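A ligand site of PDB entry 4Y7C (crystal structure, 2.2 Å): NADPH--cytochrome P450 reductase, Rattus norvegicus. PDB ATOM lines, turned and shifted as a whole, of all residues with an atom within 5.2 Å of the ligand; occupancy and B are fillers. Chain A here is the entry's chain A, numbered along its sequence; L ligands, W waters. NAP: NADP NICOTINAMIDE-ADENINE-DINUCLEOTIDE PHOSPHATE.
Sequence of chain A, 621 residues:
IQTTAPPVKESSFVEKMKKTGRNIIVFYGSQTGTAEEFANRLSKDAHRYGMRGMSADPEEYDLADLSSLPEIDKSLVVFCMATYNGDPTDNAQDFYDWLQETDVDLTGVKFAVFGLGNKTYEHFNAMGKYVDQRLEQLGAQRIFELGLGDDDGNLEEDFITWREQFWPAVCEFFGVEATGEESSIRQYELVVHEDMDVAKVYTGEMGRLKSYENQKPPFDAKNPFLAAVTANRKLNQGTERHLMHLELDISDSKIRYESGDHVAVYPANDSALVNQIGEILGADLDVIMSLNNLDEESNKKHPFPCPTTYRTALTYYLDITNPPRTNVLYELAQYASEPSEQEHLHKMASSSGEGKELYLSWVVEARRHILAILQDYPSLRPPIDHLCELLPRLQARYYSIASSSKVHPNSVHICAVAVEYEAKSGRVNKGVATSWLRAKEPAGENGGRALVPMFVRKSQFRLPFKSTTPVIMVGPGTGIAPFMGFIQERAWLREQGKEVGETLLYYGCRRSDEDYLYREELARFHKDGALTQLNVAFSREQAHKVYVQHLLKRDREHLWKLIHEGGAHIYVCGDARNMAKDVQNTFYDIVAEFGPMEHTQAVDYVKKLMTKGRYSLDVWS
OG1 of Thr 478 sits at hydrogen-bond distance from O2N of the ligand (2.6 Å).
OG of Ser 539 lies within hydrogen-bond range of O3B of the ligand, at 2.6 Å.
The guanidinium group (NH1) of Arg 241 lies within salt-bridge range of an oxygen (O1N) of the ligand (2.7 Å).
O of Cys 509 sits at hydrogen-bond distance from O3B of the ligand (3.1 Å).
The backbone NH (N) of Thr 478 is in hydrogen-bond range of an oxygen (O2N) of the ligand, at 2.6 Å.
The guanidinium group (NE) of Arg 540 is in salt-bridge range of an oxygen (O1X) of the ligand (2.8 Å).
The side-chain amino group (NZ) of Lys 545 lies within salt-bridge range of an oxygen (O1X) of the ligand, at 2.9 Å.
A nitrogen (N6A) of the ligand is in hydrogen-bond range of the side-chain carboxylate (OD2) of Asp 582 (3.2 Å).
A nitrogen (N1A) of the ligand lies within hydrogen-bond range of the side-chain amide nitrogen (NE2) of Gln 549, 3.1 Å away.
An oxygen (O2X) of the ligand sits at hydrogen-bond distance from the side-chain hydroxyl (OH) of Tyr 547, at 2.7 Å.
The guanidinium group of Arg 510 lies within salt-bridge range of the side-chain carboxylate of Asp 515.
The guanidinium group (NH2) of Arg 241 is in salt-bridge range of the side-chain carboxylate (OD2) of Asp 515 (3.2 Å).
O of Arg 510 is in hydrogen-bond range of N of Arg 540 (2.9 Å).
The backbone NH (N) of Gly 477 is in hydrogen-bond range of the backbone carbonyl oxygen (O) of Gly 508.
N of Cys 509 lies within hydrogen-bond range of O of Ala 537, 3.0 Å away.
The backbone NH (N) of Ser 539 lies within hydrogen-bond range of the backbone carbonyl oxygen (O) of Cys 509.
Water W2 bridges an oxygen (O3B) of the ligand and the backbone carbonyl oxygen (O) of Ala 537.
Water W4 lies within hydrogen-bond range of O1A of the ligand, OD2 of Asp 515, N of Arg 510 and NH2 of Arg 241.
Water W7 bridges N6A of the ligand (2.9 Å) and ND2 of Asn 578 (3.5 Å).
Water W3 lies within hydrogen-bond range of O2N of the ligand (2.9 Å) and OG1 of Thr 478 (3.4 Å).
Water W5 bridges the backbone NH (N) of Val 548 (3.0 Å) and a nitrogen (N3A) of the ligand (3.0 Å).
Pro 476 touches the ligand (CB to O4B, 3.8 Å).
Gly 477 touches the ligand (C to O2N, 3.5 Å).
Gly 508 touches the ligand (O to C4B, 3.9 Å).
N of Arg 510 touches O3B of the ligand, 3.7 Å away.
Asn 578 touches the ligand (CB to N6A, 3.6 Å).
Met 579 touches the ligand (CG to C2A, 3.6 Å).
Hydrophobic or aromatic side chains within 4 Å of the ligand: Pro 476, Tyr 547 and Met 579.
Of the 21 residues printed, 15 come within 4 Å of the ligand.
The nearest printed residue that does not touch the ligand is Val 548 (4.2 Å).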
ATOM      1  N   ARG A 241      14.200  -1.083 -19.523  1.00  0.00           N
ATOM      2  CA  ARG A 241      14.319  -1.757 -20.807  1.00  0.00           C
ATOM      3  C   ARG A 241      13.071  -2.541 -21.145  1.00  0.00           C
ATOM      4  O   ARG A 241      12.088  -2.530 -20.402  1.00  0.00           O
ATOM      5  CB  ARG A 241      15.518  -2.704 -20.760  1.00  0.00           C
ATOM      6  CG  ARG A 241      16.810  -2.043 -20.326  1.00  0.00           C
ATOM      7  CD  ARG A 241      17.953  -3.023 -20.384  1.00  0.00           C
ATOM      8  NE  ARG A 241      17.868  -4.058 -19.343  1.00  0.00           N
ATOM      9  CZ  ARG A 241      18.537  -5.211 -19.400  1.00  0.00           C
ATOM     10  NH1 ARG A 241      19.323  -5.479 -20.442  1.00  0.00           N
ATOM     11  NH2 ARG A 241      18.420  -6.087 -18.417  1.00  0.00           N
ATOM     12  N   LEU A 243      12.038  -6.390 -22.065  1.00  0.00           N
ATOM     13  CA  LEU A 243      12.361  -7.794 -22.264  1.00  0.00           C
ATOM     14  C   LEU A 243      11.031  -8.476 -22.535  1.00  0.00           C
ATOM     15  O   LEU A 243      10.030  -8.203 -21.863  1.00  0.00           O
ATOM     16  CB  LEU A 243      13.087  -8.358 -21.045  1.00  0.00           C
ATOM     17  CG  LEU A 243      14.536  -7.849 -20.965  1.00  0.00           C
ATOM     18  CD1 LEU A 243      14.582  -6.557 -20.190  1.00  0.00           C
ATOM     19  CD2 LEU A 243      15.432  -8.881 -20.317  1.00  0.00           C
ATOM     20  N   VAL A 417      15.745  -9.564 -25.327  1.00  0.00           N
ATOM     21  CA  VAL A 417      15.786  -8.170 -24.882  1.00  0.00           C
ATOM     22  C   VAL A 417      15.738  -7.304 -26.142  1.00  0.00           C
ATOM     23  O   VAL A 417      16.474  -7.537 -27.097  1.00  0.00           O
ATOM     24  CB  VAL A 417      17.063  -7.870 -24.038  1.00  0.00           C
ATOM     25  CG1 VAL A 417      18.323  -8.157 -24.837  1.00  0.00           C
ATOM     26  CG2 VAL A 417      17.050  -6.406 -23.576  1.00  0.00           C
ATOM     27  N   PRO A 476      22.463 -15.576 -16.270  1.00  0.00           N
ATOM     28  CA  PRO A 476      21.916 -14.281 -15.848  1.00  0.00           C
ATOM     29  C   PRO A 476      21.309 -13.543 -17.046  1.00  0.00           C
ATOM     30  O   PRO A 476      21.626 -13.856 -18.197  1.00  0.00           O
ATOM     31  CB  PRO A 476      23.138 -13.568 -15.284  1.00  0.00           C
ATOM     32  CG  PRO A 476      24.250 -14.101 -16.121  1.00  0.00           C
ATOM     33  CD  PRO A 476      23.928 -15.585 -16.190  1.00  0.00           C
ATOM     34  N   GLY A 477      20.427 -12.589 -16.777  1.00  0.00           N
ATOM     35  CA  GLY A 477      19.797 -11.843 -17.850  1.00  0.00           C
ATOM     36  C   GLY A 477      19.049 -12.760 -18.804  1.00  0.00           C
ATOM     37  O   GLY A 477      18.384 -13.699 -18.369  1.00  0.00           O
ATOM     38  N   THR A 478      19.148 -12.488 -20.099  1.00  0.00           N
ATOM     39  CA  THR A 478      18.468 -13.322 -21.093  1.00  0.00           C
ATOM     40  C   THR A 478      19.117 -14.707 -21.214  1.00  0.00           C
ATOM     41  O   THR A 478      18.628 -15.551 -21.952  1.00  0.00           O
ATOM     42  CB  THR A 478      18.445 -12.677 -22.500  1.00  0.00           C
ATOM     43  OG1 THR A 478      19.765 -12.224 -22.842  1.00  0.00           O
ATOM     44  CG2 THR A 478      17.454 -11.531 -22.549  1.00  0.00           C
ATOM     45  N   GLY A 479      20.209 -14.915 -20.491  1.00  0.00           N
ATOM     46  CA  GLY A 479      20.855 -16.208 -20.517  1.00  0.00           C
ATOM     47  C   GLY A 479      19.963 -17.250 -19.870  1.00  0.00           C
ATOM     48  O   GLY A 479      20.242 -18.439 -19.913  1.00  0.00           O
ATOM     49  N   GLY A 508      20.555 -14.172 -12.549  1.00  0.00           N
ATOM     50  CA  GLY A 508      20.901 -12.835 -12.102  1.00  0.00           C
ATOM     51  C   GLY A 508      20.203 -11.738 -12.893  1.00  0.00           C
ATOM     52  O   GLY A 508      19.938 -11.874 -14.082  1.00  0.00           O
ATOM     53  N   CYS A 509      19.873 -10.648 -12.218  1.00  0.00           N
ATOM     54  CA  CYS A 509      19.225  -9.525 -12.844  1.00  0.00           C
ATOM     55  C   CYS A 509      19.577  -8.289 -12.012  1.00  0.00           C
ATOM     56  O   CYS A 509      20.267  -8.411 -11.001  1.00  0.00           O
ATOM     57  CB  CYS A 509      17.697  -9.737 -12.905  1.00  0.00           C
ATOM     58  SG  CYS A 509      16.877  -9.903 -11.285  1.00  0.00           S
ATOM     59  N   ARG A 510      19.101  -7.122 -12.433  1.00  0.00           N
ATOM     60  CA  ARG A 510      19.395  -5.883 -11.721  1.00  0.00           C
ATOM     61  C   ARG A 510      18.657  -5.750 -10.378  1.00  0.00           C
ATOM     62  O   ARG A 510      19.292  -5.558  -9.339  1.00  0.00           O
ATOM     63  CB  ARG A 510      19.087  -4.698 -12.636  1.00  0.00           C
ATOM     64  CG  ARG A 510      19.803  -4.796 -13.998  1.00  0.00           C
ATOM     65  CD  ARG A 510      19.561  -3.581 -14.898  1.00  0.00           C
ATOM     66  NE  ARG A 510      20.289  -3.701 -16.155  1.00  0.00           N
ATOM     67  CZ  ARG A 510      20.313  -2.774 -17.113  1.00  0.00           C
ATOM     68  NH1 ARG A 510      19.641  -1.639 -16.970  1.00  0.00           N
ATOM     69  NH2 ARG A 510      21.041  -2.967 -18.205  1.00  0.00           N
ATOM     70  N   ASP A 515      13.816  -6.202 -13.475  1.00  0.00           N
ATOM     71  CA  ASP A 515      13.927  -7.157 -14.573  1.00  0.00           C
ATOM     72  C   ASP A 515      14.179  -8.628 -14.192  1.00  0.00           C
ATOM     73  O   ASP A 515      15.037  -9.285 -14.791  1.00  0.00           O
ATOM     74  CB  ASP A 515      15.016  -6.686 -15.543  1.00  0.00           C
ATOM     75  CG  ASP A 515      16.324  -6.348 -14.846  1.00  0.00           C
ATOM     76  OD1 ASP A 515      16.524  -6.776 -13.684  1.00  0.00           O
ATOM     77  OD2 ASP A 515      17.159  -5.650 -15.457  1.00  0.00           O
ATOM     78  N   ALA A 537      21.094 -13.583  -8.160  1.00  0.00           N
ATOM     79  CA  ALA A 537      21.970 -12.470  -7.842  1.00  0.00           C
ATOM     80  C   ALA A 537      21.340 -11.168  -8.347  1.00  0.00           C
ATOM     81  O   ALA A 537      21.152 -10.999  -9.559  1.00  0.00           O
ATOM     82  CB  ALA A 537      23.331 -12.681  -8.486  1.00  0.00           C
ATOM     83  N   SER A 539      22.115  -7.717  -8.964  1.00  0.00           N
ATOM     84  CA  SER A 539      23.294  -6.866  -9.092  1.00  0.00           C
ATOM     85  C   SER A 539      23.207  -5.427  -8.634  1.00  0.00           C
ATOM     86  O   SER A 539      24.244  -4.815  -8.360  1.00  0.00           O
ATOM     87  CB  SER A 539      23.771  -6.885 -10.538  1.00  0.00           C
ATOM     88  OG  SER A 539      22.822  -6.272 -11.388  1.00  0.00           O
ATOM     89  N   ARG A 540      22.010  -4.861  -8.557  1.00  0.00           N
ATOM     90  CA  ARG A 540      21.895  -3.451  -8.169  1.00  0.00           C
ATOM     91  C   ARG A 540      21.051  -3.140  -6.940  1.00  0.00           C
ATOM     92  O   ARG A 540      20.706  -1.979  -6.725  1.00  0.00           O
ATOM     93  CB  ARG A 540      21.394  -2.636  -9.371  1.00  0.00           C
ATOM     94  CG  ARG A 540      22.194  -2.887 -10.635  1.00  0.00           C
ATOM     95  CD  ARG A 540      21.800  -1.980 -11.802  1.00  0.00           C
ATOM     96  NE  ARG A 540      22.566  -2.303 -13.006  1.00  0.00           N
ATOM     97  CZ  ARG A 540      22.505  -1.601 -14.138  1.00  0.00           C
ATOM     98  NH1 ARG A 540      21.707  -0.550 -14.218  1.00  0.00           N
ATOM     99  NH2 ARG A 540      23.233  -1.968 -15.181  1.00  0.00           N
ATOM    100  N   LYS A 545      28.232  -4.921  -6.474  1.00  0.00           N
ATOM    101  CA  LYS A 545      27.608  -5.825  -7.431  1.00  0.00           C
ATOM    102  C   LYS A 545      27.546  -7.237  -6.862  1.00  0.00           C
ATOM    103  O   LYS A 545      28.483  -7.702  -6.204  1.00  0.00           O
ATOM    104  CB  LYS A 545      28.434  -5.883  -8.726  1.00  0.00           C
ATOM    105  CG  LYS A 545      28.584  -4.562  -9.469  1.00  0.00           C
ATOM    106  CD  LYS A 545      27.283  -4.095 -10.102  1.00  0.00           C
ATOM    107  CE  LYS A 545      27.534  -2.952 -11.074  1.00  0.00           C
ATOM    108  NZ  LYS A 545      26.296  -2.479 -11.748  1.00  0.00           N
ATOM    109  N   TYR A 547      26.889 -10.914  -8.360  1.00  0.00           N
ATOM    110  CA  TYR A 547      26.748 -11.660  -9.593  1.00  0.00           C
ATOM    111  C   TYR A 547      26.615 -13.147  -9.364  1.00  0.00           C
ATOM    112  O   TYR A 547      26.905 -13.649  -8.283  1.00  0.00           O
ATOM    113  CB  TYR A 547      27.970 -11.416 -10.491  1.00  0.00           C
ATOM    114  CG  TYR A 547      28.131  -9.994 -10.989  1.00  0.00           C
ATOM    115  CD1 TYR A 547      27.018  -9.204 -11.292  1.00  0.00           C
ATOM    116  CD2 TYR A 547      29.395  -9.478 -11.277  1.00  0.00           C
ATOM    117  CE1 TYR A 547      27.159  -7.938 -11.876  1.00  0.00           C
ATOM    118  CE2 TYR A 547      29.546  -8.212 -11.863  1.00  0.00           C
ATOM    119  CZ  TYR A 547      28.431  -7.453 -12.165  1.00  0.00           C
ATOM    120  OH  TYR A 547      28.579  -6.238 -12.795  1.00  0.00           O
ATOM    121  N   VAL A 548      26.200 -13.856 -10.410  1.00  0.00           N
ATOM    122  CA  VAL A 548      26.028 -15.289 -10.283  1.00  0.00           C
ATOM    123  C   VAL A 548      27.295 -15.992  -9.776  1.00  0.00           C
ATOM    124  O   VAL A 548      27.190 -16.865  -8.920  1.00  0.00           O
ATOM    125  CB  VAL A 548      25.571 -15.916 -11.630  1.00  0.00           C
ATOM    126  CG1 VAL A 548      24.107 -15.526 -11.913  1.00  0.00           C
ATOM    127  CG2 VAL A 548      26.467 -15.463 -12.767  1.00  0.00           C
ATOM    128  N   GLN A 549      28.465 -15.603 -10.265  1.00  0.00           N
ATOM    129  CA  GLN A 549      29.697 -16.253  -9.838  1.00  0.00           C
ATOM    130  C   GLN A 549      29.972 -16.047  -8.348  1.00  0.00           C
ATOM    131  O   GLN A 549      30.701 -16.829  -7.739  1.00  0.00           O
ATOM    132  CB  GLN A 549      30.911 -15.793 -10.657  1.00  0.00           C
ATOM    133  CG  GLN A 549      31.233 -14.306 -10.634  1.00  0.00           C
ATOM    134  CD  GLN A 549      30.571 -13.531 -11.767  1.00  0.00           C
ATOM    135  OE1 GLN A 549      29.479 -13.894 -12.220  1.00  0.00           O
ATOM    136  NE2 GLN A 549      31.228 -12.473 -12.228  1.00  0.00           N
ATOM    137  N   ASN A 578      32.087 -10.993 -20.830  1.00  0.00           N
ATOM    138  CA  ASN A 578      32.589 -10.992 -19.456  1.00  0.00           C
ATOM    139  C   ASN A 578      32.034 -12.075 -18.533  1.00  0.00           C
ATOM    140  O   ASN A 578      32.787 -12.761 -17.848  1.00  0.00           O
ATOM    141  CB  ASN A 578      32.362  -9.615 -18.826  1.00  0.00           C
ATOM    142  CG  ASN A 578      32.995  -8.477 -19.647  1.00  0.00           C
ATOM    143  OD1 ASN A 578      32.503  -8.117 -20.718  1.00  0.00           O
ATOM    144  ND2 ASN A 578      34.091  -7.930 -19.139  1.00  0.00           N
ATOM    145  N   MET A 579      30.720 -12.232 -18.526  1.00  0.00           N
ATOM    146  CA  MET A 579      30.066 -13.223 -17.661  1.00  0.00           C
ATOM    147  C   MET A 579      30.633 -14.635 -17.817  1.00  0.00           C
ATOM    148  O   MET A 579      31.038 -15.258 -16.826  1.00  0.00           O
ATOM    149  CB  MET A 579      28.566 -13.221 -17.940  1.00  0.00           C
ATOM    150  CG  MET A 579      27.716 -14.023 -16.948  1.00  0.00           C
ATOM    151  SD  MET A 579      27.767 -15.797 -17.191  1.00  0.00           S
ATOM    152  CE  MET A 579      26.816 -15.956 -18.686  1.00  0.00           C
ATOM    153  N   ASP A 582      34.231 -14.928 -16.467  1.00  0.00           N
ATOM    154  CA  ASP A 582      34.225 -14.799 -15.018  1.00  0.00           C
ATOM    155  C   ASP A 582      33.693 -16.061 -14.348  1.00  0.00           C
ATOM    156  O   ASP A 582      34.236 -16.512 -13.341  1.00  0.00           O
ATOM    157  CB  ASP A 582      33.404 -13.592 -14.557  1.00  0.00           C
ATOM    158  CG  ASP A 582      34.061 -12.274 -14.914  1.00  0.00           C
ATOM    159  OD1 ASP A 582      35.304 -12.248 -15.104  1.00  0.00           O
ATOM    160  OD2 ASP A 582      33.343 -11.253 -14.991  1.00  0.00           O
HETATM  161  PA  NAP L   1      22.092  -7.791 -18.511  1.00  0.00           P
HETATM  162  O1A NAP L   1      20.757  -7.351 -18.047  1.00  0.00           O
HETATM  163  O2A NAP L   1      22.976  -6.810 -19.175  1.00  0.00           O
HETATM  164  O5B NAP L   1      22.878  -8.465 -17.272  1.00  0.00           O
HETATM  165  C5B NAP L   1      22.214  -9.458 -16.493  1.00  0.00           C
HETATM  166  C4B NAP L   1      22.847  -9.535 -15.108  1.00  0.00           C
HETATM  167  O4B NAP L   1      24.235  -9.882 -15.269  1.00  0.00           O
HETATM  168  C3B NAP L   1      22.818  -8.148 -14.465  1.00  0.00           C
HETATM  169  O3B NAP L   1      22.568  -8.271 -13.062  1.00  0.00           O
HETATM  170  C2B NAP L   1      24.225  -7.623 -14.715  1.00  0.00           C
HETATM  171  O2B NAP L   1      24.565  -6.716 -13.654  1.00  0.00           O
HETATM  172  C1B NAP L   1      24.986  -8.923 -14.500  1.00  0.00           C
HETATM  173  N9A NAP L   1      26.399  -8.867 -14.946  1.00  0.00           N
HETATM  174  C8A NAP L   1      26.998  -7.852 -15.563  1.00  0.00           C
HETATM  175  N7A NAP L   1      28.265  -8.195 -15.761  1.00  0.00           N
HETATM  176  C5A NAP L   1      28.454  -9.420 -15.278  1.00  0.00           C
HETATM  177  C6A NAP L   1      29.536 -10.181 -15.167  1.00  0.00           C
HETATM  178  N6A NAP L   1      30.658  -9.709 -15.712  1.00  0.00           N
HETATM  179  N1A NAP L   1      29.508 -11.389 -14.603  1.00  0.00           N
HETATM  180  C2A NAP L   1      28.290 -11.877 -14.115  1.00  0.00           C
HETATM  181  N3A NAP L   1      27.168 -11.057 -14.240  1.00  0.00           N
HETATM  182  C4A NAP L   1      27.278  -9.848 -14.804  1.00  0.00           C
HETATM  183  O3  NAP L   1      21.911  -9.049 -19.488  1.00  0.00           O
HETATM  184  PN  NAP L   1      21.103  -9.128 -20.875  1.00  0.00           P
HETATM  185  O1N NAP L   1      20.214  -7.951 -20.985  1.00  0.00           O
HETATM  186  O2N NAP L   1      20.519 -10.483 -21.010  1.00  0.00           O
HETATM  187  O5D NAP L   1      22.281  -8.968 -21.950  1.00  0.00           O
HETATM  188  P2B NAP L   1      24.924  -5.172 -13.942  1.00  0.00           P
HETATM  189  O1X NAP L   1      24.397  -4.467 -12.746  1.00  0.00           O
HETATM  190  O2X NAP L   1      26.402  -5.157 -14.042  1.00  0.00           O
HETATM  191  O3X NAP L   1      24.212  -4.871 -15.199  1.00  0.00           O
HETATM  192  O   HOH W   1      25.927  -8.411 -19.452  1.00  0.00           O
HETATM  193  O   HOH W   2      23.312 -10.481 -11.586  1.00  0.00           O
HETATM  194  O   HOH W   3      22.943 -11.971 -21.746  1.00  0.00           O
HETATM  195  O   HOH W   4      19.170  -7.964 -15.680  1.00  0.00           O
HETATM  196  O   HOH W   5      24.969 -12.324 -12.616  1.00  0.00           O
HETATM  197  O   HOH W   6      25.125  -5.766 -18.148  1.00  0.00           O
HETATM  198  O   HOH W   7      32.284  -7.345 -16.237  1.00  0.00           O
HETATM  199  O   HOH W   8      25.572 -11.038 -17.849  1.00  0.00           O
